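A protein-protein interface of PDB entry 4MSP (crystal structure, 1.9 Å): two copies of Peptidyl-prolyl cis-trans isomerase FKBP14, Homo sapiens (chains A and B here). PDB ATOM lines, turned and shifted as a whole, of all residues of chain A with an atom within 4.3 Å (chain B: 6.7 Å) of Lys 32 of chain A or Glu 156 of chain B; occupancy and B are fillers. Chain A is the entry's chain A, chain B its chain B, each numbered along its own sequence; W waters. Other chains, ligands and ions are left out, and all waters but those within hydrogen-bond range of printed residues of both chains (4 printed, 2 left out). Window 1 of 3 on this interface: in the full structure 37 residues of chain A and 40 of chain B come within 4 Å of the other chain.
Among the printed residues, Asp or Glu carboxylates within 4 Å of a Lys or Arg side-chain nitrogen of the other chain: Lys 32 of chain A with Glu 156 of chain B.
N of Leu 68 of chain A lies within hydrogen-bond range of O of Asp 35 of chain A (3.0 Å). The side-chain amino group (NZ) of Lys 155 of chain B is in salt-bridge range of the side-chain carboxylate (OE2) of Glu 156 of chain B, at 2.6 Å. The side-chain carboxylate (OE2) of Glu 156 of chain B lies within salt-bridge range of the side-chain amino group (NZ) of Lys 159 of chain B (2.9 Å). The side-chain amino group (NZ) of Lys 32 of chain A sits at hydrogen-bond distance from a ring nitrogen (NE2) of His 160 of chain A (3.0 Å). N of Lys 32 of chain A lies within hydrogen-bond range of OD2 of Asp 35 of chain A, at 2.9 Å. The side-chain carboxylate of Glu 135 of chain B sits at hydrogen-bond distance from the side-chain hydroxyl of Tyr 152 of chain B, 2.7 Å away.
Water W4 lies within hydrogen-bond range of the side-chain carboxylate (OD2) of Asp 35 of chain A, the backbone carbonyl oxygen (O) of Lys 30 of chain A and the side-chain amino group (NZ) of Lys 155 of chain B. Water W3 bridges the backbone carbonyl oxygen (O) of Glu 135 of chain B and the backbone NH (N) of Lys 30 of chain A. Water W1 lies within hydrogen-bond range of OG of Ser 132 of chain B, NE2 of His 160 of chain A, OE1 of Glu 135 of chain B and OH of Tyr 152 of chain B. Water W2 lies within hydrogen-bond range of O of Lys 30 of chain A (2.7 Å) and NZ of Lys 155 of chain B (2.8 Å).
Among the printed residues, pairs that only touch across the chains: Lys 30 of chain A with Glu 135 of chain B, Lys 32 of chain A with Glu 135 of chain B, Lys 32 of chain A with Lys 155 of chain B, Lys 32 of chain A with Lys 159 of chain B, Asp 35 of chain A with Lys 159 of chain B and His 160 of chain A with Ser 132 of chain B.
Of the printed residues of chain B, Lys 30 of chain A touches Glu 135. Of chain B, only Glu 135, Tyr 152, Lys 155, Glu 156 and Lys 159 come within 4 Å of Lys 32 of chain A. Printed residues of chain B within 4 Å of His 160 of chain A: Ser 132 and Tyr 152. Of the printed residues of chain A, Ser 132 of chain B touches His 160 (3.9 Å). Of chain A, only Lys 32 (3.0 Å) comes within 4 Å of Glu 156 of chain B. Gly 161 of chain B touches none of the printed residues of chain A. Ala 162 of chain B touches none of the printed residues of chain A. The nearest residue of chain B that does not touch Lys 32 of chain A is Ser 132 of chain B (6.1 Å). The nearest printed residue of chain B that does not touch Asp 35 of chain A is Lys 155 of chain B (5.0 Å).
Position printed for both chains: 160.
A ring nitrogen (NE2) of His 160 of chain A sits close to the side-chain hydroxyl (OH) of Tyr 152 of chain B. The side-chain carboxylate (OE1) of Glu 156 of chain B lies within salt-bridge range of the side-chain amino group (NZ) of Lys 32 of chain A, 3.0 Å away. OH of Tyr 152 of chain B lies within hydrogen-bond range of NZ of Lys 32 of chain A (3.0 Å).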
ATOM      1  N   LYS A  30     -15.744  24.501 -10.655  1.00  0.00           N
ATOM      2  CA  LYS A  30     -16.079  25.890 -10.370  1.00  0.00           C
ATOM      3  C   LYS A  30     -17.587  26.083 -10.255  1.00  0.00           C
ATOM      4  O   LYS A  30     -18.351  25.421 -10.951  1.00  0.00           O
ATOM      5  CB  LYS A  30     -15.519  26.805 -11.466  1.00  0.00           C
ATOM      6  CG  LYS A  30     -13.989  26.874 -11.463  1.00  0.00           C
ATOM      7  CD  LYS A  30     -13.491  27.926 -12.436  1.00  0.00           C
ATOM      8  CE  LYS A  30     -11.983  27.936 -12.512  1.00  0.00           C
ATOM      9  NZ  LYS A  30     -11.436  28.965 -13.434  1.00  0.00           N
ATOM     10  N   THR A  31     -18.014  27.022  -9.408  1.00  0.00           N
ATOM     11  CA  THR A  31     -19.442  27.268  -9.218  1.00  0.00           C
ATOM     12  C   THR A  31     -20.107  27.835 -10.465  1.00  0.00           C
ATOM     13  O   THR A  31     -19.512  28.628 -11.217  1.00  0.00           O
ATOM     14  CB  THR A  31     -19.725  28.235  -8.056  1.00  0.00           C
ATOM     15  OG1 THR A  31     -19.090  29.491  -8.312  1.00  0.00           O
ATOM     16  CG2 THR A  31     -19.208  27.665  -6.739  1.00  0.00           C
ATOM     17  N   LYS A  32     -21.359  27.425 -10.656  1.00  0.00           N
ATOM     18  CA  LYS A  32     -22.172  27.767 -11.820  1.00  0.00           C
ATOM     19  C   LYS A  32     -23.613  27.892 -11.345  1.00  0.00           C
ATOM     20  O   LYS A  32     -23.998  27.223 -10.395  1.00  0.00           O
ATOM     21  CB  LYS A  32     -22.078  26.625 -12.836  1.00  0.00           C
ATOM     22  CG  LYS A  32     -22.896  26.823 -14.079  1.00  0.00           C
ATOM     23  CD  LYS A  32     -22.735  25.655 -15.050  1.00  0.00           C
ATOM     24  CE  LYS A  32     -23.558  25.914 -16.314  1.00  0.00           C
ATOM     25  NZ  LYS A  32     -23.334  24.871 -17.342  1.00  0.00           N
ATOM     26  N   GLY A  33     -24.405  28.746 -11.990  1.00  0.00           N
ATOM     27  CA  GLY A  33     -25.795  28.938 -11.603  1.00  0.00           C
ATOM     28  C   GLY A  33     -26.519  27.631 -11.327  1.00  0.00           C
ATOM     29  O   GLY A  33     -26.409  26.669 -12.099  1.00  0.00           O
ATOM     30  N   GLY A  34     -27.224  27.579 -10.203  1.00  0.00           N
ATOM     31  CA  GLY A  34     -27.916  26.365  -9.806  1.00  0.00           C
ATOM     32  C   GLY A  34     -27.197  25.525  -8.755  1.00  0.00           C
ATOM     33  O   GLY A  34     -27.836  24.751  -8.045  1.00  0.00           O
ATOM     34  N   ASP A  35     -25.874  25.652  -8.659  1.00  0.00           N
ATOM     35  CA  ASP A  35     -25.105  24.860  -7.706  1.00  0.00           C
ATOM     36  C   ASP A  35     -25.474  25.220  -6.270  1.00  0.00           C
ATOM     37  O   ASP A  35     -25.817  26.363  -5.965  1.00  0.00           O
ATOM     38  CB  ASP A  35     -23.597  25.116  -7.848  1.00  0.00           C
ATOM     39  CG  ASP A  35     -22.993  24.496  -9.081  1.00  0.00           C
ATOM     40  OD1 ASP A  35     -23.637  23.618  -9.698  1.00  0.00           O
ATOM     41  OD2 ASP A  35     -21.847  24.888  -9.421  1.00  0.00           O
ATOM     42  N   LEU A  68     -26.550  29.297  -5.860  1.00  0.00           N
ATOM     43  CA  LEU A  68     -26.020  30.359  -6.706  1.00  0.00           C
ATOM     44  C   LEU A  68     -26.959  30.673  -7.876  1.00  0.00           C
ATOM     45  O   LEU A  68     -27.505  29.769  -8.503  1.00  0.00           O
ATOM     46  CB  LEU A  68     -24.645  29.941  -7.254  1.00  0.00           C
ATOM     47  CG  LEU A  68     -23.930  30.935  -8.176  1.00  0.00           C
ATOM     48  CD1 LEU A  68     -23.574  32.228  -7.409  1.00  0.00           C
ATOM     49  CD2 LEU A  68     -22.678  30.299  -8.782  1.00  0.00           C
ATOM     50  N   HIS A 160     -21.978  25.820 -24.698  1.00  0.00           N
ATOM     51  CA  HIS A 160     -20.621  25.697 -24.170  1.00  0.00           C
ATOM     52  C   HIS A 160     -19.574  25.424 -25.247  1.00  0.00           C
ATOM     53  O   HIS A 160     -18.450  25.027 -24.946  1.00  0.00           O
ATOM     54  CB  HIS A 160     -20.578  24.638 -23.064  1.00  0.00           C
ATOM     55  CG  HIS A 160     -21.504  24.947 -21.930  1.00  0.00           C
ATOM     56  ND1 HIS A 160     -22.858  24.691 -21.985  1.00  0.00           N
ATOM     57  CD2 HIS A 160     -21.284  25.550 -20.738  1.00  0.00           C
ATOM     58  CE1 HIS A 160     -23.429  25.103 -20.866  1.00  0.00           C
ATOM     59  NE2 HIS A 160     -22.494  25.627 -20.092  1.00  0.00           N
ATOM     60  N   SER B 132     -18.554  30.844 -19.260  1.00  0.00           N
ATOM     61  CA  SER B 132     -18.506  29.409 -19.540  1.00  0.00           C
ATOM     62  C   SER B 132     -17.071  28.915 -19.698  1.00  0.00           C
ATOM     63  O   SER B 132     -16.707  27.861 -19.173  1.00  0.00           O
ATOM     64  CB  SER B 132     -19.352  29.063 -20.776  1.00  0.00           C
ATOM     65  OG  SER B 132     -20.712  29.397 -20.529  1.00  0.00           O
ATOM     66  N   GLU B 135     -15.413  28.811 -16.246  1.00  0.00           N
ATOM     67  CA  GLU B 135     -15.908  27.637 -15.520  1.00  0.00           C
ATOM     68  C   GLU B 135     -15.143  26.368 -15.877  1.00  0.00           C
ATOM     69  O   GLU B 135     -14.847  25.530 -15.016  1.00  0.00           O
ATOM     70  CB  GLU B 135     -17.392  27.405 -15.831  1.00  0.00           C
ATOM     71  CG  GLU B 135     -18.308  28.365 -15.158  1.00  0.00           C
ATOM     72  CD  GLU B 135     -19.714  28.320 -15.749  1.00  0.00           C
ATOM     73  OE1 GLU B 135     -19.993  27.406 -16.557  1.00  0.00           O
ATOM     74  OE2 GLU B 135     -20.510  29.214 -15.415  1.00  0.00           O
ATOM     75  N   ALA B 151     -13.948  16.582 -17.329  1.00  0.00           N
ATOM     76  CA  ALA B 151     -14.415  16.840 -15.970  1.00  0.00           C
ATOM     77  C   ALA B 151     -15.701  17.654 -15.959  1.00  0.00           C
ATOM     78  O   ALA B 151     -16.606  17.376 -15.167  1.00  0.00           O
ATOM     79  CB  ALA B 151     -13.327  17.528 -15.127  1.00  0.00           C
ATOM     80  N   TYR B 152     -15.771  18.652 -16.837  1.00  0.00           N
ATOM     81  CA  TYR B 152     -16.944  19.499 -16.967  1.00  0.00           C
ATOM     82  C   TYR B 152     -18.155  18.682 -17.443  1.00  0.00           C
ATOM     83  O   TYR B 152     -19.242  18.799 -16.889  1.00  0.00           O
ATOM     84  CB  TYR B 152     -16.667  20.641 -17.948  1.00  0.00           C
ATOM     85  CG  TYR B 152     -17.669  21.786 -17.885  1.00  0.00           C
ATOM     86  CD1 TYR B 152     -17.619  22.721 -16.863  1.00  0.00           C
ATOM     87  CD2 TYR B 152     -18.646  21.937 -18.865  1.00  0.00           C
ATOM     88  CE1 TYR B 152     -18.515  23.779 -16.806  1.00  0.00           C
ATOM     89  CE2 TYR B 152     -19.555  22.999 -18.819  1.00  0.00           C
ATOM     90  CZ  TYR B 152     -19.483  23.911 -17.791  1.00  0.00           C
ATOM     91  OH  TYR B 152     -20.373  24.967 -17.736  1.00  0.00           O
ATOM     92  N   LEU B 153     -17.958  17.877 -18.483  1.00  0.00           N
ATOM     93  CA  LEU B 153     -19.026  17.015 -18.995  1.00  0.00           C
ATOM     94  C   LEU B 153     -19.544  16.057 -17.919  1.00  0.00           C
ATOM     95  O   LEU B 153     -20.750  15.822 -17.799  1.00  0.00           O
ATOM     96  CB  LEU B 153     -18.539  16.206 -20.202  1.00  0.00           C
ATOM     97  CG  LEU B 153     -18.442  16.968 -21.525  1.00  0.00           C
ATOM     98  CD1 LEU B 153     -17.631  16.174 -22.535  1.00  0.00           C
ATOM     99  CD2 LEU B 153     -19.825  17.275 -22.072  1.00  0.00           C
ATOM    100  N   LYS B 154     -18.620  15.518 -17.141  1.00  0.00           N
ATOM    101  CA  LYS B 154     -18.954  14.572 -16.086  1.00  0.00           C
ATOM    102  C   LYS B 154     -19.855  15.228 -15.055  1.00  0.00           C
ATOM    103  O   LYS B 154     -20.903  14.683 -14.708  1.00  0.00           O
ATOM    104  CB  LYS B 154     -17.686  14.055 -15.416  1.00  0.00           C
ATOM    105  CG  LYS B 154     -17.918  13.054 -14.296  1.00  0.00           C
ATOM    106  CD  LYS B 154     -16.590  12.586 -13.717  1.00  0.00           C
ATOM    107  CE  LYS B 154     -16.737  11.306 -12.899  1.00  0.00           C
ATOM    108  NZ  LYS B 154     -17.701  11.471 -11.788  1.00  0.00           N
ATOM    109  N   LYS B 155     -19.458  16.394 -14.547  1.00  0.00           N
ATOM    110  CA  LYS B 155     -20.257  17.009 -13.497  1.00  0.00           C
ATOM    111  C   LYS B 155     -21.558  17.582 -14.050  1.00  0.00           C
ATOM    112  O   LYS B 155     -22.560  17.596 -13.352  1.00  0.00           O
ATOM    113  CB  LYS B 155     -19.459  18.037 -12.663  1.00  0.00           C
ATOM    114  CG  LYS B 155     -19.029  19.293 -13.414  1.00  0.00           C
ATOM    115  CD  LYS B 155     -20.039  20.422 -13.224  1.00  0.00           C
ATOM    116  CE  LYS B 155     -19.521  21.723 -13.806  1.00  0.00           C
ATOM    117  NZ  LYS B 155     -20.557  22.776 -13.747  1.00  0.00           N
ATOM    118  N   GLU B 156     -21.549  18.036 -15.304  1.00  0.00           N
ATOM    119  CA  GLU B 156     -22.768  18.569 -15.908  1.00  0.00           C
ATOM    120  C   GLU B 156     -23.831  17.483 -16.071  1.00  0.00           C
ATOM    121  O   GLU B 156     -25.019  17.712 -15.827  1.00  0.00           O
ATOM    122  CB  GLU B 156     -22.478  19.248 -17.243  1.00  0.00           C
ATOM    123  CG  GLU B 156     -21.858  20.616 -17.096  1.00  0.00           C
ATOM    124  CD  GLU B 156     -22.798  21.629 -16.467  1.00  0.00           C
ATOM    125  OE1 GLU B 156     -23.831  21.960 -17.085  1.00  0.00           O
ATOM    126  OE2 GLU B 156     -22.503  22.104 -15.351  1.00  0.00           O
ATOM    127  N   PHE B 157     -23.396  16.292 -16.455  1.00  0.00           N
ATOM    128  CA  PHE B 157     -24.301  15.152 -16.495  1.00  0.00           C
ATOM    129  C   PHE B 157     -24.768  14.752 -15.100  1.00  0.00           C
ATOM    130  O   PHE B 157     -25.971  14.571 -14.848  1.00  0.00           O
ATOM    131  CB  PHE B 157     -23.631  13.965 -17.207  1.00  0.00           C
ATOM    132  CG  PHE B 157     -23.880  13.951 -18.688  1.00  0.00           C
ATOM    133  CD1 PHE B 157     -23.473  15.011 -19.476  1.00  0.00           C
ATOM    134  CD2 PHE B 157     -24.561  12.903 -19.283  1.00  0.00           C
ATOM    135  CE1 PHE B 157     -23.712  15.022 -20.830  1.00  0.00           C
ATOM    136  CE2 PHE B 157     -24.809  12.908 -20.639  1.00  0.00           C
ATOM    137  CZ  PHE B 157     -24.386  13.970 -21.414  1.00  0.00           C
ATOM    138  N   GLU B 158     -23.810  14.621 -14.191  1.00  0.00           N
ATOM    139  CA  GLU B 158     -24.114  14.129 -12.858  1.00  0.00           C
ATOM    140  C   GLU B 158     -25.028  15.089 -12.106  1.00  0.00           C
ATOM    141  O   GLU B 158     -25.773  14.667 -11.217  1.00  0.00           O
ATOM    142  CB  GLU B 158     -22.831  13.876 -12.075  1.00  0.00           C
ATOM    143  CG  GLU B 158     -22.106  12.611 -12.499  1.00  0.00           C
ATOM    144  CD  GLU B 158     -20.736  12.494 -11.865  1.00  0.00           C
ATOM    145  OE1 GLU B 158     -20.286  13.482 -11.236  1.00  0.00           O
ATOM    146  OE2 GLU B 158     -20.109  11.419 -12.004  1.00  0.00           O
ATOM    147  N   LYS B 159     -24.962  16.371 -12.468  1.00  0.00           N
ATOM    148  CA  LYS B 159     -25.827  17.403 -11.880  1.00  0.00           C
ATOM    149  C   LYS B 159     -27.272  17.024 -12.088  1.00  0.00           C
ATOM    150  O   LYS B 159     -28.090  17.087 -11.173  1.00  0.00           O
ATOM    151  CB  LYS B 159     -25.629  18.756 -12.574  1.00  0.00           C
ATOM    152  CG  LYS B 159     -24.516  19.614 -12.035  1.00  0.00           C
ATOM    153  CD  LYS B 159     -24.688  21.070 -12.457  1.00  0.00           C
ATOM    154  CE  LYS B 159     -25.335  21.220 -13.829  1.00  0.00           C
ATOM    155  NZ  LYS B 159     -25.144  22.600 -14.371  1.00  0.00           N
ATOM    156  N   HIS B 160     -27.580  16.655 -13.324  1.00  0.00           N
ATOM    157  CA  HIS B 160     -28.937  16.309 -13.702  1.00  0.00           C
ATOM    158  C   HIS B 160     -29.272  14.872 -13.314  1.00  0.00           C
ATOM    159  O   HIS B 160     -30.347  14.377 -13.631  1.00  0.00           O
ATOM    160  CB  HIS B 160     -29.140  16.506 -15.207  1.00  0.00           C
ATOM    161  CG  HIS B 160     -28.965  17.922 -15.668  1.00  0.00           C
ATOM    162  ND1 HIS B 160     -29.992  18.843 -15.648  1.00  0.00           N
ATOM    163  CD2 HIS B 160     -27.891  18.568 -16.183  1.00  0.00           C
ATOM    164  CE1 HIS B 160     -29.556  19.997 -16.123  1.00  0.00           C
ATOM    165  NE2 HIS B 160     -28.282  19.859 -16.451  1.00  0.00           N
ATOM    166  N   GLY B 161     -28.349  14.207 -12.623  1.00  0.00           N
ATOM    167  CA  GLY B 161     -28.542  12.816 -12.252  1.00  0.00           C
ATOM    168  C   GLY B 161     -28.482  11.919 -13.479  1.00  0.00           C
ATOM    169  O   GLY B 161     -29.067  10.830 -13.490  1.00  0.00           O
ATOM    170  N   ALA B 162     -27.782  12.382 -14.516  1.00  0.00           N
ATOM    171  CA  ALA B 162     -27.595  11.604 -15.740  1.00  0.00           C
ATOM    172  C   ALA B 162     -26.310  10.783 -15.666  1.00  0.00           C
ATOM    173  O   ALA B 162     -25.237  11.328 -15.411  1.00  0.00           O
ATOM    174  CB  ALA B 162     -27.569  12.520 -16.954  1.00  0.00           C
HETATM  175  O   HOH W   1     -21.968  27.943 -18.612  1.00  0.00           O
HETATM  176  O   HOH W   2     -18.637  24.876 -13.603  1.00  0.00           O
HETATM  177  O   HOH W   3     -16.187  23.827 -13.430  1.00  0.00           O
HETATM  178  O   HOH W   4     -20.287  23.481 -10.919  1.00  0.00           O
